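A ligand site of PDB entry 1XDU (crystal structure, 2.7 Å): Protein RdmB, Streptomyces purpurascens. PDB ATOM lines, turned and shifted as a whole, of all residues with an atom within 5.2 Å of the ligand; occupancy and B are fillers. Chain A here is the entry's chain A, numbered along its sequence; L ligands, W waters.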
ATOM      1  N   TRP A 146       8.317 -10.343  -9.873  1.00  0.00           N
ATOM      2  CA  TRP A 146       9.059  -9.672  -8.804  1.00  0.00           C
ATOM      3  C   TRP A 146       8.728  -8.192  -8.668  1.00  0.00           C
ATOM      4  O   TRP A 146       8.799  -7.649  -7.574  1.00  0.00           O
ATOM      5  CB  TRP A 146      10.561  -9.869  -8.983  1.00  0.00           C
ATOM      6  CG  TRP A 146      10.995 -11.253  -8.690  1.00  0.00           C
ATOM      7  CD1 TRP A 146      11.518 -12.154  -9.573  1.00  0.00           C
ATOM      8  CD2 TRP A 146      10.927 -11.930  -7.432  1.00  0.00           C
ATOM      9  NE1 TRP A 146      11.794 -13.338  -8.926  1.00  0.00           N
ATOM     10  CE2 TRP A 146      11.440 -13.223  -7.613  1.00  0.00           C
ATOM     11  CE3 TRP A 146      10.493 -11.557  -6.152  1.00  0.00           C
ATOM     12  CZ2 TRP A 146      11.524 -14.149  -6.564  1.00  0.00           C
ATOM     13  CZ3 TRP A 146      10.580 -12.468  -5.122  1.00  0.00           C
ATOM     14  CH2 TRP A 146      11.085 -13.752  -5.339  1.00  0.00           C
ATOM     15  N   CYS A 165      14.111 -20.479   2.941  1.00  0.00           N
ATOM     16  CA  CYS A 165      15.161 -19.472   3.049  1.00  0.00           C
ATOM     17  C   CYS A 165      14.733 -18.312   3.963  1.00  0.00           C
ATOM     18  O   CYS A 165      15.561 -17.493   4.374  1.00  0.00           O
ATOM     19  CB  CYS A 165      15.553 -18.953   1.664  1.00  0.00           C
ATOM     20  SG  CYS A 165      16.744 -20.013   0.814  1.00  0.00           S
ATOM     21  N   TYR A 171      20.791 -19.374   6.287  1.00  0.00           N
ATOM     22  CA  TYR A 171      22.020 -18.971   5.613  1.00  0.00           C
ATOM     23  C   TYR A 171      23.286 -19.315   6.380  1.00  0.00           C
ATOM     24  O   TYR A 171      24.381 -18.981   5.936  1.00  0.00           O
ATOM     25  CB  TYR A 171      21.962 -17.463   5.304  1.00  0.00           C
ATOM     26  CG  TYR A 171      20.923 -17.130   4.268  1.00  0.00           C
ATOM     27  CD1 TYR A 171      19.726 -16.512   4.610  1.00  0.00           C
ATOM     28  CD2 TYR A 171      21.124 -17.481   2.938  1.00  0.00           C
ATOM     29  CE1 TYR A 171      18.766 -16.226   3.641  1.00  0.00           C
ATOM     30  CE2 TYR A 171      20.173 -17.205   1.968  1.00  0.00           C
ATOM     31  CZ  TYR A 171      19.000 -16.580   2.329  1.00  0.00           C
ATOM     32  OH  TYR A 171      18.058 -16.315   1.357  1.00  0.00           O
ATOM     33  N   ASP A 188      25.703  -7.314  -3.057  1.00  0.00           N
ATOM     34  CA  ASP A 188      24.673  -8.339  -2.963  1.00  0.00           C
ATOM     35  C   ASP A 188      23.578  -7.986  -3.960  1.00  0.00           C
ATOM     36  O   ASP A 188      22.676  -7.196  -3.664  1.00  0.00           O
ATOM     37  CB  ASP A 188      24.168  -8.414  -1.525  1.00  0.00           C
ATOM     38  CG  ASP A 188      23.227  -9.569  -1.265  1.00  0.00           C
ATOM     39  OD1 ASP A 188      23.020 -10.425  -2.163  1.00  0.00           O
ATOM     40  OD2 ASP A 188      22.633  -9.712  -0.177  1.00  0.00           O
ATOM     41  N   VAL A 189      23.667  -8.562  -5.152  1.00  0.00           N
ATOM     42  CA  VAL A 189      22.800  -8.187  -6.283  1.00  0.00           C
ATOM     43  C   VAL A 189      21.462  -8.912  -6.246  1.00  0.00           C
ATOM     44  O   VAL A 189      21.408 -10.128  -6.406  1.00  0.00           O
ATOM     45  CB  VAL A 189      23.513  -8.457  -7.623  1.00  0.00           C
ATOM     46  CG1 VAL A 189      22.600  -8.142  -8.802  1.00  0.00           C
ATOM     47  CG2 VAL A 189      24.807  -7.637  -7.717  1.00  0.00           C
ATOM     48  N   GLY A 190      20.386  -8.151  -6.068  1.00  0.00           N
ATOM     49  CA  GLY A 190      19.064  -8.711  -5.856  1.00  0.00           C
ATOM     50  C   GLY A 190      19.034  -9.476  -4.552  1.00  0.00           C
ATOM     51  O   GLY A 190      18.508 -10.585  -4.488  1.00  0.00           O
ATOM     52  N   GLY A 191      19.611  -8.878  -3.515  1.00  0.00           N
ATOM     53  CA  GLY A 191      19.849  -9.553  -2.247  1.00  0.00           C
ATOM     54  C   GLY A 191      18.624  -9.797  -1.377  1.00  0.00           C
ATOM     55  O   GLY A 191      18.767 -10.222  -0.229  1.00  0.00           O
ATOM     56  N   GLY A 192      17.445  -9.539  -1.908  1.00  0.00           N
ATOM     57  CA  GLY A 192      16.204  -9.797  -1.206  1.00  0.00           C
ATOM     58  C   GLY A 192      16.114  -8.957   0.049  1.00  0.00           C
ATOM     59  O   GLY A 192      16.318  -7.752  -0.014  1.00  0.00           O
ATOM     60  N   MET A 196      21.682 -13.595   3.553  1.00  0.00           N
ATOM     61  CA  MET A 196      23.078 -13.959   3.304  1.00  0.00           C
ATOM     62  C   MET A 196      24.055 -12.891   3.803  1.00  0.00           C
ATOM     63  O   MET A 196      24.977 -13.201   4.545  1.00  0.00           O
ATOM     64  CB  MET A 196      23.313 -14.225   1.812  1.00  0.00           C
ATOM     65  CG  MET A 196      24.536 -15.082   1.506  1.00  0.00           C
ATOM     66  SD  MET A 196      24.834 -16.429   2.677  1.00  0.00           S
ATOM     67  CE  MET A 196      26.565 -16.815   2.330  1.00  0.00           C
ATOM     68  N   VAL A 212      21.408  -4.446  -3.461  1.00  0.00           N
ATOM     69  CA  VAL A 212      20.643  -3.837  -4.544  1.00  0.00           C
ATOM     70  C   VAL A 212      19.321  -4.559  -4.726  1.00  0.00           C
ATOM     71  O   VAL A 212      19.286  -5.761  -4.976  1.00  0.00           O
ATOM     72  CB  VAL A 212      21.441  -3.854  -5.869  1.00  0.00           C
ATOM     73  CG1 VAL A 212      20.557  -3.476  -7.052  1.00  0.00           C
ATOM     74  CG2 VAL A 212      22.624  -2.910  -5.757  1.00  0.00           C
ATOM     75  N   GLU A 213      18.221  -3.832  -4.582  1.00  0.00           N
ATOM     76  CA  GLU A 213      16.907  -4.443  -4.651  1.00  0.00           C
ATOM     77  C   GLU A 213      15.820  -3.483  -5.152  1.00  0.00           C
ATOM     78  O   GLU A 213      16.035  -2.281  -5.257  1.00  0.00           O
ATOM     79  CB  GLU A 213      16.529  -4.994  -3.275  1.00  0.00           C
ATOM     80  CG  GLU A 213      16.723  -6.497  -3.136  1.00  0.00           C
ATOM     81  CD  GLU A 213      15.748  -7.308  -3.975  1.00  0.00           C
ATOM     82  OE1 GLU A 213      14.757  -6.731  -4.467  1.00  0.00           O
ATOM     83  OE2 GLU A 213      15.953  -8.522  -4.145  1.00  0.00           O
ATOM     84  N   LEU A 214      14.666  -4.027  -5.465  1.00  0.00           N
ATOM     85  CA  LEU A 214      13.491  -3.233  -5.778  1.00  0.00           C
ATOM     86  C   LEU A 214      12.967  -2.662  -4.455  1.00  0.00           C
ATOM     87  O   LEU A 214      13.344  -3.134  -3.395  1.00  0.00           O
ATOM     88  CB  LEU A 214      12.445  -4.096  -6.505  1.00  0.00           C
ATOM     89  CG  LEU A 214      12.999  -4.932  -7.676  1.00  0.00           C
ATOM     90  CD1 LEU A 214      11.901  -5.773  -8.295  1.00  0.00           C
ATOM     91  CD2 LEU A 214      13.661  -4.043  -8.723  1.00  0.00           C
ATOM     92  N   PRO A 217      11.696  -5.314  -1.152  1.00  0.00           N
ATOM     93  CA  PRO A 217      12.742  -5.969  -0.359  1.00  0.00           C
ATOM     94  C   PRO A 217      13.802  -5.003   0.164  1.00  0.00           C
ATOM     95  O   PRO A 217      14.450  -5.285   1.173  1.00  0.00           O
ATOM     96  CB  PRO A 217      13.370  -6.961  -1.345  1.00  0.00           C
ATOM     97  CG  PRO A 217      12.347  -7.154  -2.382  1.00  0.00           C
ATOM     98  CD  PRO A 217      11.674  -5.823  -2.535  1.00  0.00           C
ATOM     99  N   GLY A 239      17.403  -0.243  -6.983  1.00  0.00           N
ATOM    100  CA  GLY A 239      17.957  -0.331  -8.317  1.00  0.00           C
ATOM    101  C   GLY A 239      17.549  -1.527  -9.151  1.00  0.00           C
ATOM    102  O   GLY A 239      17.106  -2.563  -8.625  1.00  0.00           O
ATOM    103  N   ASP A 240      17.705  -1.389 -10.462  1.00  0.00           N
ATOM    104  CA  ASP A 240      17.420  -2.435 -11.438  1.00  0.00           C
ATOM    105  C   ASP A 240      18.745  -3.110 -11.787  1.00  0.00           C
ATOM    106  O   ASP A 240      19.663  -2.452 -12.268  1.00  0.00           O
ATOM    107  CB  ASP A 240      16.790  -1.785 -12.679  1.00  0.00           C
ATOM    108  CG  ASP A 240      16.319  -2.802 -13.725  1.00  0.00           C
ATOM    109  OD1 ASP A 240      16.283  -4.009 -13.444  1.00  0.00           O
ATOM    110  OD2 ASP A 240      15.972  -2.451 -14.869  1.00  0.00           O
ATOM    111  N   PHE A 241      18.868  -4.420 -11.529  1.00  0.00           N
ATOM    112  CA  PHE A 241      20.123  -5.140 -11.807  1.00  0.00           C
ATOM    113  C   PHE A 241      20.329  -5.459 -13.299  1.00  0.00           C
ATOM    114  O   PHE A 241      21.336  -6.078 -13.671  1.00  0.00           O
ATOM    115  CB  PHE A 241      20.321  -6.395 -10.915  1.00  0.00           C
ATOM    116  CG  PHE A 241      19.229  -7.452 -11.004  1.00  0.00           C
ATOM    117  CD1 PHE A 241      18.618  -7.789 -12.202  1.00  0.00           C
ATOM    118  CD2 PHE A 241      18.863  -8.154  -9.862  1.00  0.00           C
ATOM    119  CE1 PHE A 241      17.638  -8.773 -12.251  1.00  0.00           C
ATOM    120  CE2 PHE A 241      17.884  -9.147  -9.908  1.00  0.00           C
ATOM    121  CZ  PHE A 241      17.276  -9.453 -11.107  1.00  0.00           C
ATOM    122  N   PHE A 242      19.370  -5.054 -14.128  1.00  0.00           N
ATOM    123  CA  PHE A 242      19.563  -5.052 -15.570  1.00  0.00           C
ATOM    124  C   PHE A 242      20.282  -3.763 -15.989  1.00  0.00           C
ATOM    125  O   PHE A 242      21.018  -3.758 -16.978  1.00  0.00           O
ATOM    126  CB  PHE A 242      18.221  -5.210 -16.279  1.00  0.00           C
ATOM    127  CG  PHE A 242      17.581  -6.559 -16.057  1.00  0.00           C
ATOM    128  CD1 PHE A 242      16.399  -6.675 -15.321  1.00  0.00           C
ATOM    129  CD2 PHE A 242      18.172  -7.710 -16.559  1.00  0.00           C
ATOM    130  CE1 PHE A 242      15.826  -7.916 -15.106  1.00  0.00           C
ATOM    131  CE2 PHE A 242      17.594  -8.954 -16.352  1.00  0.00           C
ATOM    132  CZ  PHE A 242      16.421  -9.062 -15.624  1.00  0.00           C
ATOM    133  N   SER A 255      22.667 -14.569  -4.757  1.00  0.00           N
ATOM    134  CA  SER A 255      22.073 -15.602  -3.907  1.00  0.00           C
ATOM    135  C   SER A 255      20.626 -15.863  -4.330  1.00  0.00           C
ATOM    136  O   SER A 255      19.761 -15.019  -4.102  1.00  0.00           O
ATOM    137  CB  SER A 255      22.129 -15.161  -2.447  1.00  0.00           C
ATOM    138  OG  SER A 255      21.323 -15.979  -1.609  1.00  0.00           O
ATOM    139  N   PHE A 256      20.368 -17.024  -4.925  1.00  0.00           N
ATOM    140  CA  PHE A 256      19.046 -17.418  -5.424  1.00  0.00           C
ATOM    141  C   PHE A 256      18.428 -16.366  -6.341  1.00  0.00           C
ATOM    142  O   PHE A 256      17.281 -15.953  -6.152  1.00  0.00           O
ATOM    143  CB  PHE A 256      18.112 -17.752  -4.243  1.00  0.00           C
ATOM    144  CG  PHE A 256      18.614 -18.881  -3.411  1.00  0.00           C
ATOM    145  CD1 PHE A 256      19.179 -18.650  -2.171  1.00  0.00           C
ATOM    146  CD2 PHE A 256      18.553 -20.172  -3.894  1.00  0.00           C
ATOM    147  CE1 PHE A 256      19.664 -19.697  -1.408  1.00  0.00           C
ATOM    148  CE2 PHE A 256      19.035 -21.232  -3.135  1.00  0.00           C
ATOM    149  CZ  PHE A 256      19.604 -20.988  -1.891  1.00  0.00           C
ATOM    150  N   VAL A 257      19.198 -15.961  -7.338  1.00  0.00           N
ATOM    151  CA  VAL A 257      18.783 -14.974  -8.331  1.00  0.00           C
ATOM    152  C   VAL A 257      18.769 -15.569  -9.723  1.00  0.00           C
ATOM    153  O   VAL A 257      17.782 -15.474 -10.433  1.00  0.00           O
ATOM    154  CB  VAL A 257      19.710 -13.744  -8.327  1.00  0.00           C
ATOM    155  CG1 VAL A 257      19.353 -12.778  -9.458  1.00  0.00           C
ATOM    156  CG2 VAL A 257      19.648 -13.035  -6.992  1.00  0.00           C
ATOM    157  N   LEU A 259      18.404 -18.510 -10.900  1.00  0.00           N
ATOM    158  CA  LEU A 259      17.283 -19.426 -11.133  1.00  0.00           C
ATOM    159  C   LEU A 259      15.959 -18.741 -11.524  1.00  0.00           C
ATOM    160  O   LEU A 259      15.091 -19.363 -12.130  1.00  0.00           O
ATOM    161  CB  LEU A 259      17.055 -20.340  -9.924  1.00  0.00           C
ATOM    162  CG  LEU A 259      16.227 -19.823  -8.740  1.00  0.00           C
ATOM    163  CD1 LEU A 259      16.059 -20.916  -7.672  1.00  0.00           C
ATOM    164  CD2 LEU A 259      16.856 -18.578  -8.119  1.00  0.00           C
ATOM    165  N   ASN A 260      15.796 -17.464 -11.170  1.00  0.00           N
ATOM    166  CA  ASN A 260      14.581 -16.730 -11.498  1.00  0.00           C
ATOM    167  C   ASN A 260      14.463 -16.294 -12.972  1.00  0.00           C
ATOM    168  O   ASN A 260      13.458 -15.701 -13.350  1.00  0.00           O
ATOM    169  CB  ASN A 260      14.451 -15.489 -10.586  1.00  0.00           C
ATOM    170  CG  ASN A 260      14.320 -15.842  -9.101  1.00  0.00           C
ATOM    171  OD1 ASN A 260      14.665 -15.039  -8.232  1.00  0.00           O
ATOM    172  ND2 ASN A 260      13.809 -17.042  -8.805  1.00  0.00           N
ATOM    173  N   TRP A 261      15.463 -16.617 -13.791  1.00  0.00           N
ATOM    174  CA  TRP A 261      15.595 -16.014 -15.123  1.00  0.00           C
ATOM    175  C   TRP A 261      16.003 -16.991 -16.215  1.00  0.00           C
ATOM    176  O   TRP A 261      16.692 -17.973 -15.967  1.00  0.00           O
ATOM    177  CB  TRP A 261      16.619 -14.888 -15.067  1.00  0.00           C
ATOM    178  CG  TRP A 261      16.263 -13.837 -14.083  1.00  0.00           C
ATOM    179  CD1 TRP A 261      16.778 -13.689 -12.832  1.00  0.00           C
ATOM    180  CD2 TRP A 261      15.290 -12.794 -14.255  1.00  0.00           C
ATOM    181  NE1 TRP A 261      16.197 -12.614 -12.211  1.00  0.00           N
ATOM    182  CE2 TRP A 261      15.284 -12.042 -13.055  1.00  0.00           C
ATOM    183  CE3 TRP A 261      14.430 -12.419 -15.292  1.00  0.00           C
ATOM    184  CZ2 TRP A 261      14.443 -10.935 -12.864  1.00  0.00           C
ATOM    185  CZ3 TRP A 261      13.597 -11.313 -15.105  1.00  0.00           C
ATOM    186  CH2 TRP A 261      13.615 -10.579 -13.902  1.00  0.00           C
HETATM  187  N1  LIG L   1      19.218 -12.847  -2.876  1.00  0.00           N
HETATM  188  C1  LIG L   1      17.901 -13.321  -2.466  1.00  0.00           C
HETATM  189  C2  LIG L   1      18.071 -14.509  -1.557  1.00  0.00           C
HETATM  190  O1  LIG L   1      19.046 -14.590  -0.832  1.00  0.00           O
HETATM  191  O2  LIG L   1      17.163 -15.479  -1.544  1.00  0.00           O
HETATM  192  C3  LIG L   1      17.095 -13.688  -3.717  1.00  0.00           C
HETATM  193  C4  LIG L   1      15.602 -13.370  -3.589  1.00  0.00           C
HETATM  194  C5  LIG L   1      14.822 -13.627  -4.897  1.00  0.00           C
HETATM  195  N2  LIG L   1      14.945 -15.024  -5.256  1.00  0.00           N
HETATM  196  C6  LIG L   1      15.269 -12.744  -6.081  1.00  0.00           C
HETATM  197  C7  LIG L   1      15.293 -11.242  -5.751  1.00  0.00           C
HETATM  198  O3  LIG L   1      15.805 -10.376  -6.772  1.00  0.00           O
HETATM  199  C8  LIG L   1      13.910 -10.738  -5.365  1.00  0.00           C
HETATM  200  O4  LIG L   1      13.920 -10.419  -3.980  1.00  0.00           O
HETATM  201  C9  LIG L   1      13.636  -9.511  -6.201  1.00  0.00           C
HETATM  202  O5  LIG L   1      13.235  -8.398  -5.433  1.00  0.00           O
HETATM  203  C10 LIG L   1      14.921  -9.258  -6.988  1.00  0.00           C
HETATM  204  N3  LIG L   1      14.660  -8.791  -8.374  1.00  0.00           N
HETATM  205  C11 LIG L   1      13.778  -9.261  -9.285  1.00  0.00           C
HETATM  206  N4  LIG L   1      13.787  -8.537 -10.451  1.00  0.00           N
HETATM  207  C12 LIG L   1      14.696  -7.570 -10.279  1.00  0.00           C
HETATM  208  C13 LIG L   1      15.270  -6.436 -11.043  1.00  0.00           C
HETATM  209  N5  LIG L   1      14.835  -6.210 -12.296  1.00  0.00           N
HETATM  210  N6  LIG L   1      16.232  -5.659 -10.466  1.00  0.00           N
HETATM  211  C14 LIG L   1      16.686  -5.869  -9.205  1.00  0.00           C
HETATM  212  N7  LIG L   1      16.237  -6.866  -8.432  1.00  0.00           N
HETATM  213  C15 LIG L   1      15.215  -7.743  -8.949  1.00  0.00           C
HETATM  214  O   HOH W   1      21.870 -11.598  -4.197  1.00  0.00           O
HETATM  215  O   HOH W   2      13.274 -17.821  -6.036  1.00  0.00           O
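An oxygen (O5) of the ligand lies within hydrogen-bond range of the side-chain carboxylate (OE1) of Glu 213, at 2.5 Å.
O of Ser 255 lies within hydrogen-bond range of N1 of the ligand, at 2.6 Å.
OG of Ser 255 lies within hydrogen-bond range of O1 of the ligand, 2.8 Å away.
O of Phe 256 lies within hydrogen-bond range of N2 of the ligand (2.7 Å).
The backbone carbonyl oxygen of Gly 190 sits at hydrogen-bond distance from a nitrogen (N1) of the ligand, 2.9 Å away.
The side-chain carboxylate (OD1) of Asp 240 sits at hydrogen-bond distance from a nitrogen (N5) of the ligand (2.9 Å).
An oxygen (O1) of the ligand sits at hydrogen-bond distance from the side-chain hydroxyl (OH) of Tyr 171 (3.0 Å).
The side-chain amide oxygen of Asn 260 is in hydrogen-bond range of a nitrogen (N2) of the ligand (3.0 Å).
The backbone NH (N) of Phe 241 sits at hydrogen-bond distance from a nitrogen (N6) of the ligand, 3.1 Å away.
Merely in contact with the ligand: Trp 146 (3.3 Å), Gly 191 (3.4 Å), Gly 192 (3.6 Å), Leu 214 (3.5 Å), Pro 217 (3.4 Å), Gly 239 (3.4 Å), Phe 242 (3.4 Å) and Trp 261 (3.5 Å).
Along chain A the residues within 4 Å of the ligand span positions 146 to 261.
The backbone NH of Gly 239 sits at hydrogen-bond distance from the backbone carbonyl oxygen of Glu 213 (3.0 Å).
The backbone NH (N) of Gly 192 sits at hydrogen-bond distance from the side-chain carboxylate (OE2) of Glu 213 (2.9 Å).
The side-chain amide oxygen (OD1) of Asn 260 lies close to the backbone carbonyl oxygen (O) of Phe 256 (3.5 Å).
N of Gly 190 is in hydrogen-bond range of O of Val 212 (2.8 Å).
OD1 of Asp 240 sits close to N of Phe 242, 3.3 Å away.
The side-chain amide oxygen of Asn 260 sits at hydrogen-bond distance from the indole nitrogen of Trp 146 (3.4 Å).
The backbone carbonyl oxygen (O) of Val 212 lies within hydrogen-bond range of the backbone NH (N) of Gly 191, 3.5 Å away.
Water W1 lies within hydrogen-bond range of OD1 of Asp 188 (2.6 Å), O of Val 189 (2.7 Å), N of Ser 255 (3.1 Å) and N1 of the ligand (3.2 Å).
Water W2 lies within hydrogen-bond range of the side-chain amide nitrogen (ND2) of Asn 260 (2.9 Å) and a nitrogen (N2) of the ligand (3.4 Å).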
